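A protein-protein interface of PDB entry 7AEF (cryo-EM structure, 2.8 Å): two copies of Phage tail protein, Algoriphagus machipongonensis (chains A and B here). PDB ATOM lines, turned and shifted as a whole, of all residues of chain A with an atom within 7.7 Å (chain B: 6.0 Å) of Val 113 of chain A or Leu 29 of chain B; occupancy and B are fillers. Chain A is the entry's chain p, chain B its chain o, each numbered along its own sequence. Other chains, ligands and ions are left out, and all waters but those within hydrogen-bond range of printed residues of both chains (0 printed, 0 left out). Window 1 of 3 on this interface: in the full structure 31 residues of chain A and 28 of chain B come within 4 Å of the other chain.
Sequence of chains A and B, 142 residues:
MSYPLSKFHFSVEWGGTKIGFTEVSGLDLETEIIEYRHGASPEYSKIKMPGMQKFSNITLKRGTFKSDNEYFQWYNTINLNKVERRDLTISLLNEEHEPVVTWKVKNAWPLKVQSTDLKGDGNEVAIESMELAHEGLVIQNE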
ATOM      1  N   ASN A  69      19.875  -0.048 -19.646  1.00  0.00           N
ATOM      2  CA  ASN A  69      20.681   0.760 -20.544  1.00  0.00           C
ATOM      3  C   ASN A  69      21.283   1.945 -19.778  1.00  0.00           C
ATOM      4  O   ASN A  69      21.522   3.012 -20.355  1.00  0.00           O
ATOM      5  CB  ASN A  69      19.819   1.199 -21.723  1.00  0.00           C
ATOM      6  CG  ASN A  69      20.579   1.565 -22.981  1.00  0.00           C
ATOM      7  OD1 ASN A  69      21.642   1.008 -23.261  1.00  0.00           O
ATOM      8  ND2 ASN A  69      20.033   2.457 -23.763  1.00  0.00           N
ATOM      9  N   GLU A  70      21.634   1.712 -18.527  1.00  0.00           N
ATOM     10  CA  GLU A  70      22.152   2.746 -17.650  1.00  0.00           C
ATOM     11  C   GLU A  70      23.430   3.418 -18.110  1.00  0.00           C
ATOM     12  O   GLU A  70      23.612   4.598 -17.874  1.00  0.00           O
ATOM     13  CB  GLU A  70      22.392   2.162 -16.274  1.00  0.00           C
ATOM     14  CG  GLU A  70      21.157   1.603 -15.621  1.00  0.00           C
ATOM     15  CD  GLU A  70      20.158   2.675 -15.307  1.00  0.00           C
ATOM     16  OE1 GLU A  70      19.761   3.391 -16.247  1.00  0.00           O
ATOM     17  OE2 GLU A  70      19.769   2.807 -14.137  1.00  0.00           O
ATOM     18  N   TYR A  71      24.332   2.662 -18.713  1.00  0.00           N
ATOM     19  CA  TYR A  71      25.613   3.231 -19.171  1.00  0.00           C
ATOM     20  C   TYR A  71      25.456   4.224 -20.308  1.00  0.00           C
ATOM     21  O   TYR A  71      26.071   5.299 -20.313  1.00  0.00           O
ATOM     22  CB  TYR A  71      26.585   2.158 -19.686  1.00  0.00           C
ATOM     23  CG  TYR A  71      27.434   1.379 -18.692  1.00  0.00           C
ATOM     24  CD1 TYR A  71      28.364   0.500 -19.212  1.00  0.00           C
ATOM     25  CD2 TYR A  71      27.340   1.534 -17.317  1.00  0.00           C
ATOM     26  CE1 TYR A  71      29.184  -0.200 -18.398  1.00  0.00           C
ATOM     27  CE2 TYR A  71      28.187   0.820 -16.502  1.00  0.00           C
ATOM     28  CZ  TYR A  71      29.109  -0.042 -17.052  1.00  0.00           C
ATOM     29  OH  TYR A  71      29.960  -0.742 -16.257  1.00  0.00           O
ATOM     30  N   PHE A  72      24.638   3.852 -21.282  1.00  0.00           N
ATOM     31  CA  PHE A  72      24.385   4.691 -22.430  1.00  0.00           C
ATOM     32  C   PHE A  72      23.698   5.959 -22.004  1.00  0.00           C
ATOM     33  O   PHE A  72      24.060   7.043 -22.452  1.00  0.00           O
ATOM     34  CB  PHE A  72      23.574   3.982 -23.498  1.00  0.00           C
ATOM     35  CG  PHE A  72      23.339   4.845 -24.693  1.00  0.00           C
ATOM     36  CD1 PHE A  72      24.343   5.059 -25.609  1.00  0.00           C
ATOM     37  CD2 PHE A  72      22.126   5.459 -24.894  1.00  0.00           C
ATOM     38  CE1 PHE A  72      24.139   5.869 -26.692  1.00  0.00           C
ATOM     39  CE2 PHE A  72      21.922   6.268 -25.974  1.00  0.00           C
ATOM     40  CZ  PHE A  72      22.927   6.474 -26.872  1.00  0.00           C
ATOM     41  N   GLN A  73      22.671   5.832 -21.163  1.00  0.00           N
ATOM     42  CA  GLN A  73      21.909   6.989 -20.750  1.00  0.00           C
ATOM     43  C   GLN A  73      22.758   8.035 -20.031  1.00  0.00           C
ATOM     44  O   GLN A  73      22.561   9.224 -20.249  1.00  0.00           O
ATOM     45  CB  GLN A  73      20.769   6.540 -19.858  1.00  0.00           C
ATOM     46  CG  GLN A  73      19.674   5.773 -20.585  1.00  0.00           C
ATOM     47  CD  GLN A  73      18.693   5.193 -19.622  1.00  0.00           C
ATOM     48  OE1 GLN A  73      18.951   5.214 -18.422  1.00  0.00           O
ATOM     49  NE2 GLN A  73      17.582   4.676 -20.116  1.00  0.00           N
ATOM     50  N   TRP A  74      23.697   7.623 -19.172  1.00  0.00           N
ATOM     51  CA  TRP A  74      24.566   8.594 -18.510  1.00  0.00           C
ATOM     52  C   TRP A  74      25.467   9.282 -19.553  1.00  0.00           C
ATOM     53  O   TRP A  74      25.626  10.510 -19.557  1.00  0.00           O
ATOM     54  CB  TRP A  74      25.385   7.939 -17.384  1.00  0.00           C
ATOM     55  CG  TRP A  74      26.203   8.917 -16.502  1.00  0.00           C
ATOM     56  CD1 TRP A  74      26.105  10.274 -16.449  1.00  0.00           C
ATOM     57  CD2 TRP A  74      27.216   8.575 -15.532  1.00  0.00           C
ATOM     58  NE1 TRP A  74      26.982  10.772 -15.547  1.00  0.00           N
ATOM     59  CE2 TRP A  74      27.660   9.767 -14.975  1.00  0.00           C
ATOM     60  CE3 TRP A  74      27.776   7.384 -15.106  1.00  0.00           C
ATOM     61  CZ2 TRP A  74      28.636   9.804 -14.005  1.00  0.00           C
ATOM     62  CZ3 TRP A  74      28.751   7.423 -14.137  1.00  0.00           C
ATOM     63  CH2 TRP A  74      29.171   8.607 -13.602  1.00  0.00           C
ATOM     64  N   TYR A  75      26.085   8.490 -20.435  1.00  0.00           N
ATOM     65  CA  TYR A  75      26.977   8.998 -21.477  1.00  0.00           C
ATOM     66  C   TYR A  75      26.260  10.033 -22.337  1.00  0.00           C
ATOM     67  O   TYR A  75      26.795  11.088 -22.680  1.00  0.00           O
ATOM     68  CB  TYR A  75      27.501   7.866 -22.343  1.00  0.00           C
ATOM     69  CG  TYR A  75      28.544   8.299 -23.327  1.00  0.00           C
ATOM     70  CD1 TYR A  75      29.854   8.418 -22.903  1.00  0.00           C
ATOM     71  CD2 TYR A  75      28.217   8.593 -24.630  1.00  0.00           C
ATOM     72  CE1 TYR A  75      30.825   8.819 -23.754  1.00  0.00           C
ATOM     73  CE2 TYR A  75      29.200   9.003 -25.495  1.00  0.00           C
ATOM     74  CZ  TYR A  75      30.502   9.116 -25.055  1.00  0.00           C
ATOM     75  OH  TYR A  75      31.480   9.522 -25.909  1.00  0.00           O
ATOM     76  N   ASN A  76      25.014   9.748 -22.654  1.00  0.00           N
ATOM     77  CA  ASN A  76      24.192  10.569 -23.513  1.00  0.00           C
ATOM     78  C   ASN A  76      23.732  11.889 -22.848  1.00  0.00           C
ATOM     79  O   ASN A  76      23.012  12.664 -23.472  1.00  0.00           O
ATOM     80  CB  ASN A  76      23.016   9.737 -23.995  1.00  0.00           C
ATOM     81  CG  ASN A  76      22.342  10.232 -25.233  1.00  0.00           C
ATOM     82  OD1 ASN A  76      22.990  10.538 -26.241  1.00  0.00           O
ATOM     83  ND2 ASN A  76      21.041  10.306 -25.193  1.00  0.00           N
ATOM     84  N   PRO A 110      31.498  10.026 -17.533  1.00  0.00           N
ATOM     85  CA  PRO A 110      32.095   9.027 -18.432  1.00  0.00           C
ATOM     86  C   PRO A 110      32.786   9.505 -19.723  1.00  0.00           C
ATOM     87  O   PRO A 110      32.219  10.171 -20.550  1.00  0.00           O
ATOM     88  CB  PRO A 110      30.910   8.122 -18.777  1.00  0.00           C
ATOM     89  CG  PRO A 110      29.691   8.907 -18.490  1.00  0.00           C
ATOM     90  CD  PRO A 110      30.038  10.115 -17.680  1.00  0.00           C
ATOM     91  N   LEU A 111      34.044   9.117 -19.843  1.00  0.00           N
ATOM     92  CA  LEU A 111      34.956   9.332 -20.963  1.00  0.00           C
ATOM     93  C   LEU A 111      34.659   8.435 -22.178  1.00  0.00           C
ATOM     94  O   LEU A 111      34.665   8.880 -23.309  1.00  0.00           O
ATOM     95  CB  LEU A 111      36.382   9.132 -20.464  1.00  0.00           C
ATOM     96  CG  LEU A 111      37.603   9.313 -21.342  1.00  0.00           C
ATOM     97  CD1 LEU A 111      38.772   9.633 -20.444  1.00  0.00           C
ATOM     98  CD2 LEU A 111      37.891   8.046 -22.114  1.00  0.00           C
ATOM     99  N   LYS A 112      34.384   7.158 -21.923  1.00  0.00           N
ATOM    100  CA  LYS A 112      34.071   6.189 -22.996  1.00  0.00           C
ATOM    101  C   LYS A 112      33.205   5.050 -22.463  1.00  0.00           C
ATOM    102  O   LYS A 112      33.281   4.730 -21.260  1.00  0.00           O
ATOM    103  CB  LYS A 112      35.354   5.657 -23.643  1.00  0.00           C
ATOM    104  CG  LYS A 112      36.311   4.942 -22.699  1.00  0.00           C
ATOM    105  CD  LYS A 112      37.521   4.358 -23.400  1.00  0.00           C
ATOM    106  CE  LYS A 112      38.338   5.398 -24.136  1.00  0.00           C
ATOM    107  NZ  LYS A 112      39.510   4.794 -24.814  1.00  0.00           N
ATOM    108  N   VAL A 113      32.378   4.524 -23.359  1.00  0.00           N
ATOM    109  CA  VAL A 113      31.527   3.359 -23.146  1.00  0.00           C
ATOM    110  C   VAL A 113      31.867   2.328 -24.215  1.00  0.00           C
ATOM    111  O   VAL A 113      31.830   2.622 -25.407  1.00  0.00           O
ATOM    112  CB  VAL A 113      30.027   3.727 -23.177  1.00  0.00           C
ATOM    113  CG1 VAL A 113      29.164   2.483 -22.985  1.00  0.00           C
ATOM    114  CG2 VAL A 113      29.731   4.708 -22.070  1.00  0.00           C
ATOM    115  N   GLN A 114      32.288   1.131 -23.782  1.00  0.00           N
ATOM    116  CA  GLN A 114      32.665   0.029 -24.717  1.00  0.00           C
ATOM    117  C   GLN A 114      31.696  -1.156 -24.661  1.00  0.00           C
ATOM    118  O   GLN A 114      31.444  -1.710 -23.599  1.00  0.00           O
ATOM    119  CB  GLN A 114      34.115  -0.421 -24.536  1.00  0.00           C
ATOM    120  CG  GLN A 114      35.093   0.656 -24.973  1.00  0.00           C
ATOM    121  CD  GLN A 114      36.525   0.205 -25.063  1.00  0.00           C
ATOM    122  OE1 GLN A 114      36.968  -0.662 -24.325  1.00  0.00           O
ATOM    123  NE2 GLN A 114      37.272   0.808 -25.971  1.00  0.00           N
ATOM    124  N   SER A 115      31.176  -1.502 -25.824  1.00  0.00           N
ATOM    125  CA  SER A 115      30.293  -2.657 -26.007  1.00  0.00           C
ATOM    126  C   SER A 115      31.070  -3.941 -26.262  1.00  0.00           C
ATOM    127  O   SER A 115      32.277  -3.925 -26.542  1.00  0.00           O
ATOM    128  CB  SER A 115      29.322  -2.425 -27.145  1.00  0.00           C
ATOM    129  OG  SER A 115      28.448  -1.376 -26.864  1.00  0.00           O
ATOM    130  N   GLU A 128      29.950  -5.485 -20.748  1.00  0.00           N
ATOM    131  CA  GLU A 128      30.126  -4.089 -21.143  1.00  0.00           C
ATOM    132  C   GLU A 128      30.993  -3.348 -20.125  1.00  0.00           C
ATOM    133  O   GLU A 128      30.990  -3.690 -18.931  1.00  0.00           O
ATOM    134  CB  GLU A 128      28.776  -3.388 -21.281  1.00  0.00           C
ATOM    135  CG  GLU A 128      27.915  -3.393 -20.021  1.00  0.00           C
ATOM    136  CD  GLU A 128      26.658  -2.595 -20.171  1.00  0.00           C
ATOM    137  OE1 GLU A 128      26.463  -2.010 -21.208  1.00  0.00           O
ATOM    138  OE2 GLU A 128      25.893  -2.559 -19.249  1.00  0.00           O
ATOM    139  N   SER A 129      31.669  -2.282 -20.579  1.00  0.00           N
ATOM    140  CA  SER A 129      32.505  -1.494 -19.672  1.00  0.00           C
ATOM    141  C   SER A 129      32.502   0.018 -19.896  1.00  0.00           C
ATOM    142  O   SER A 129      32.215   0.535 -20.978  1.00  0.00           O
ATOM    143  CB  SER A 129      33.931  -1.971 -19.771  1.00  0.00           C
ATOM    144  OG  SER A 129      34.471  -1.703 -21.013  1.00  0.00           O
ATOM    145  N   MET A 130      32.850   0.734 -18.832  1.00  0.00           N
ATOM    146  CA  MET A 130      32.915   2.192 -18.818  1.00  0.00           C
ATOM    147  C   MET A 130      34.184   2.762 -18.177  1.00  0.00           C
ATOM    148  O   MET A 130      34.671   2.265 -17.159  1.00  0.00           O
ATOM    149  CB  MET A 130      31.670   2.703 -18.085  1.00  0.00           C
ATOM    150  CG  MET A 130      31.573   4.201 -17.877  1.00  0.00           C
ATOM    151  SD  MET A 130      30.059   4.681 -17.016  1.00  0.00           S
ATOM    152  CE  MET A 130      28.892   4.815 -18.318  1.00  0.00           C
ATOM    153  N   GLU A 131      34.695   3.853 -18.758  1.00  0.00           N
ATOM    154  CA  GLU A 131      35.857   4.568 -18.210  1.00  0.00           C
ATOM    155  C   GLU A 131      35.484   5.980 -17.739  1.00  0.00           C
ATOM    156  O   GLU A 131      34.922   6.785 -18.500  1.00  0.00           O
ATOM    157  CB  GLU A 131      36.983   4.614 -19.243  1.00  0.00           C
ATOM    158  CG  GLU A 131      38.267   5.284 -18.786  1.00  0.00           C
ATOM    159  CD  GLU A 131      39.342   5.199 -19.845  1.00  0.00           C
ATOM    160  OE1 GLU A 131      39.125   4.492 -20.793  1.00  0.00           O
ATOM    161  OE2 GLU A 131      40.368   5.846 -19.727  1.00  0.00           O
ATOM    162  N   LEU B  27      32.088  -1.756 -31.739  1.00  0.00           N
ATOM    163  CA  LEU B  27      30.945  -0.900 -31.390  1.00  0.00           C
ATOM    164  C   LEU B  27      31.204   0.004 -30.162  1.00  0.00           C
ATOM    165  O   LEU B  27      30.568  -0.139 -29.121  1.00  0.00           O
ATOM    166  CB  LEU B  27      29.744  -1.828 -31.132  1.00  0.00           C
ATOM    167  CG  LEU B  27      29.311  -2.749 -32.344  1.00  0.00           C
ATOM    168  CD1 LEU B  27      28.242  -3.730 -31.897  1.00  0.00           C
ATOM    169  CD2 LEU B  27      28.760  -1.896 -33.477  1.00  0.00           C
ATOM    170  N   ASP B  28      32.145   0.940 -30.323  1.00  0.00           N
ATOM    171  CA  ASP B  28      32.618   1.874 -29.286  1.00  0.00           C
ATOM    172  C   ASP B  28      32.193   3.340 -29.465  1.00  0.00           C
ATOM    173  O   ASP B  28      31.934   3.789 -30.581  1.00  0.00           O
ATOM    174  CB  ASP B  28      34.138   1.857 -29.243  1.00  0.00           C
ATOM    175  CG  ASP B  28      34.741   0.546 -28.820  1.00  0.00           C
ATOM    176  OD1 ASP B  28      34.291  -0.022 -27.860  1.00  0.00           O
ATOM    177  OD2 ASP B  28      35.664   0.111 -29.474  1.00  0.00           O
ATOM    178  N   LEU B  29      32.176   4.086 -28.351  1.00  0.00           N
ATOM    179  CA  LEU B  29      31.901   5.533 -28.294  1.00  0.00           C
ATOM    180  C   LEU B  29      33.012   6.229 -27.492  1.00  0.00           C
ATOM    181  O   LEU B  29      33.361   5.744 -26.417  1.00  0.00           O
ATOM    182  CB  LEU B  29      30.563   5.768 -27.573  1.00  0.00           C
ATOM    183  CG  LEU B  29      29.290   5.121 -28.196  1.00  0.00           C
ATOM    184  CD1 LEU B  29      28.141   5.239 -27.236  1.00  0.00           C
ATOM    185  CD2 LEU B  29      28.930   5.804 -29.460  1.00  0.00           C
ATOM    186  N   GLU B  30      33.541   7.376 -27.949  1.00  0.00           N
ATOM    187  CA  GLU B  30      34.613   8.053 -27.189  1.00  0.00           C
ATOM    188  C   GLU B  30      34.575   9.596 -27.218  1.00  0.00           C
ATOM    189  O   GLU B  30      34.304  10.207 -28.249  1.00  0.00           O
ATOM    190  CB  GLU B  30      35.958   7.556 -27.707  1.00  0.00           C
ATOM    191  CG  GLU B  30      37.170   8.068 -26.983  1.00  0.00           C
ATOM    192  CD  GLU B  30      38.429   7.472 -27.523  1.00  0.00           C
ATOM    193  OE1 GLU B  30      38.344   6.584 -28.322  1.00  0.00           O
ATOM    194  OE2 GLU B  30      39.480   7.938 -27.180  1.00  0.00           O
ATOM    195  N   THR B  31      34.860  10.228 -26.070  1.00  0.00           N
ATOM    196  CA  THR B  31      34.894  11.699 -25.949  1.00  0.00           C
ATOM    197  C   THR B  31      36.239  12.211 -25.405  1.00  0.00           C
ATOM    198  O   THR B  31      36.784  11.641 -24.461  1.00  0.00           O
ATOM    199  CB  THR B  31      33.747  12.204 -25.032  1.00  0.00           C
ATOM    200  OG1 THR B  31      32.498  11.785 -25.564  1.00  0.00           O
ATOM    201  CG2 THR B  31      33.728  13.730 -24.966  1.00  0.00           C
ATOM    202  N   LYS B  54      34.428  11.034 -31.005  1.00  0.00           N
ATOM    203  CA  LYS B  54      34.933  10.050 -31.967  1.00  0.00           C
ATOM    204  C   LYS B  54      34.150   8.743 -32.021  1.00  0.00           C
ATOM    205  O   LYS B  54      33.488   8.336 -31.056  1.00  0.00           O
ATOM    206  CB  LYS B  54      36.361   9.668 -31.634  1.00  0.00           C
ATOM    207  CG  LYS B  54      37.373  10.747 -31.769  1.00  0.00           C
ATOM    208  CD  LYS B  54      38.725  10.286 -31.247  1.00  0.00           C
ATOM    209  CE  LYS B  54      38.765  10.365 -29.719  1.00  0.00           C
ATOM    210  NZ  LYS B  54      40.116  10.067 -29.150  1.00  0.00           N
ATOM    211  N   PHE B  55      34.289   8.047 -33.151  1.00  0.00           N
ATOM    212  CA  PHE B  55      33.742   6.707 -33.319  1.00  0.00           C
ATOM    213  C   PHE B  55      34.812   5.767 -33.865  1.00  0.00           C
ATOM    214  O   PHE B  55      35.677   6.194 -34.625  1.00  0.00           O
ATOM    215  CB  PHE B  55      32.562   6.721 -34.273  1.00  0.00           C
ATOM    216  CG  PHE B  55      31.451   7.561 -33.803  1.00  0.00           C
ATOM    217  CD1 PHE B  55      31.295   8.839 -34.285  1.00  0.00           C
ATOM    218  CD2 PHE B  55      30.585   7.106 -32.842  1.00  0.00           C
ATOM    219  CE1 PHE B  55      30.305   9.639 -33.821  1.00  0.00           C
ATOM    220  CE2 PHE B  55      29.591   7.912 -32.378  1.00  0.00           C
ATOM    221  CZ  PHE B  55      29.453   9.178 -32.862  1.00  0.00           C
ATOM    222  N   SER B  56      34.741   4.487 -33.507  1.00  0.00           N
ATOM    223  CA  SER B  56      35.657   3.465 -34.037  1.00  0.00           C
ATOM    224  C   SER B  56      35.124   2.820 -35.312  1.00  0.00           C
ATOM    225  O   SER B  56      33.912   2.806 -35.549  1.00  0.00           O
ATOM    226  CB  SER B  56      35.902   2.373 -33.013  1.00  0.00           C
ATOM    227  OG  SER B  56      36.570   2.861 -31.885  1.00  0.00           O
ATOM    228  N   LEU B 137      26.628   6.215 -33.906  1.00  0.00           N
ATOM    229  CA  LEU B 137      26.049   5.045 -33.264  1.00  0.00           C
ATOM    230  C   LEU B 137      25.080   5.360 -32.124  1.00  0.00           C
ATOM    231  O   LEU B 137      25.403   6.103 -31.202  1.00  0.00           O
ATOM    232  CB  LEU B 137      27.199   4.150 -32.742  1.00  0.00           C
ATOM    233  CG  LEU B 137      26.829   2.935 -31.832  1.00  0.00           C
ATOM    234  CD1 LEU B 137      26.016   1.923 -32.589  1.00  0.00           C
ATOM    235  CD2 LEU B 137      28.129   2.280 -31.315  1.00  0.00           C
ATOM    236  N   VAL B 138      23.902   4.743 -32.191  1.00  0.00           N
ATOM    237  CA  VAL B 138      22.859   4.832 -31.169  1.00  0.00           C
ATOM    238  C   VAL B 138      22.536   3.443 -30.606  1.00  0.00           C
ATOM    239  O   VAL B 138      22.385   2.476 -31.355  1.00  0.00           O
ATOM    240  CB  VAL B 138      21.589   5.510 -31.720  1.00  0.00           C
ATOM    241  CG1 VAL B 138      20.483   5.535 -30.676  1.00  0.00           C
ATOM    242  CG2 VAL B 138      21.921   6.924 -32.133  1.00  0.00           C
ATOM    243  N   ILE B 139      22.470   3.322 -29.278  1.00  0.00           N
ATOM    244  CA  ILE B 139      22.198   2.021 -28.666  1.00  0.00           C
ATOM    245  C   ILE B 139      20.811   1.947 -28.033  1.00  0.00           C
ATOM    246  O   ILE B 139      20.470   2.745 -27.164  1.00  0.00           O
ATOM    247  CB  ILE B 139      23.254   1.692 -27.600  1.00  0.00           C
ATOM    248  CG1 ILE B 139      24.643   1.707 -28.261  1.00  0.00           C
ATOM    249  CG2 ILE B 139      22.955   0.279 -27.006  1.00  0.00           C
ATOM    250  CD1 ILE B 139      25.815   1.640 -27.325  1.00  0.00           C
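Among the printed residues, pairs that only touch across the chains: Phe 72 of chain A with Ile 139 of chain B (3.9 Å), Tyr 75 of chain A with Leu 29 of chain B (3.96 Å), Tyr 75 of chain A with Glu 30 of chain B (3.4 Å), Leu 111 of chain A with Glu 30 of chain B (3.97 Å), Lys 112 of chain A with Leu 29 of chain B (3.4 Å) and Gln 114 of chain A with Asp 28 of chain B (3.1 Å).
No position is printed for both chains. Of the 12 pairs that touch across the chains among the printed residues, none has its exchanged pair printed and touching as well.
Printed residues of chain A within 4 Å of Leu 29 of chain B: Tyr 75 (3.96 Å), Lys 112 (3.4 Å) and Val 113 (3.3 Å). Printed residues of chain B within 4 Å of Leu 111 of chain A: Glu 30 (3.97 Å) and Thr 31 (3.1 Å). Of the printed residues of chain A, Thr 31 of chain B touches Tyr 75 and Leu 111. Of the printed residues of chain A, Glu 30 of chain B touches Tyr 75, Leu 111 and Lys 112. Lys 54 of chain B touches none of the printed residues of chain A.
The side-chain carboxylate of Glu 30 of chain B lies within salt-bridge range of the side-chain amino group of Lys 54 of chain B, 3.0 Å away. The backbone carbonyl oxygen (O) of Ser 129 of chain A is in hydrogen-bond range of the backbone NH (N) of Gln 114 of chain A. The backbone carbonyl oxygen (O) of Lys 112 of chain A lies within hydrogen-bond range of the backbone NH (N) of Glu 131 of chain A, 3.0 Å away. O of Glu 131 of chain A sits at hydrogen-bond distance from N of Leu 111 of chain A.
Of the 11 printed residues of chain B, 6 touch a printed residue of chain A. Among the printed residues, 12 pairs touch across the chains. Among the printed residues, Asp or Glu carboxylates within 4 Å of a Lys or Arg side-chain nitrogen of the other chain: Lys 112 of chain A with Glu 30 of chain B (3.9 Å).
OG1 of Thr 31 of chain B lies within hydrogen-bond range of OH of Tyr 75 of chain A, 2.5 Å away. O of Leu 111 of chain A lies within hydrogen-bond range of N of Thr 31 of chain B (3.1 Å). OG of Ser 115 of chain A lies close to O of Leu 27 of chain B (3.3 Å). OE2 of Glu 30 of chain B lies within salt-bridge range of NZ of Lys 112 of chain A (3.9 Å). N of Leu 29 of chain B is in hydrogen-bond range of O of Val 113 of chain A (3.3 Å). The backbone carbonyl oxygen (O) of Ile 139 of chain B lies within hydrogen-bond range of the side-chain amide nitrogen (ND2) of Asn 69 of chain A, 3.4 Å away.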
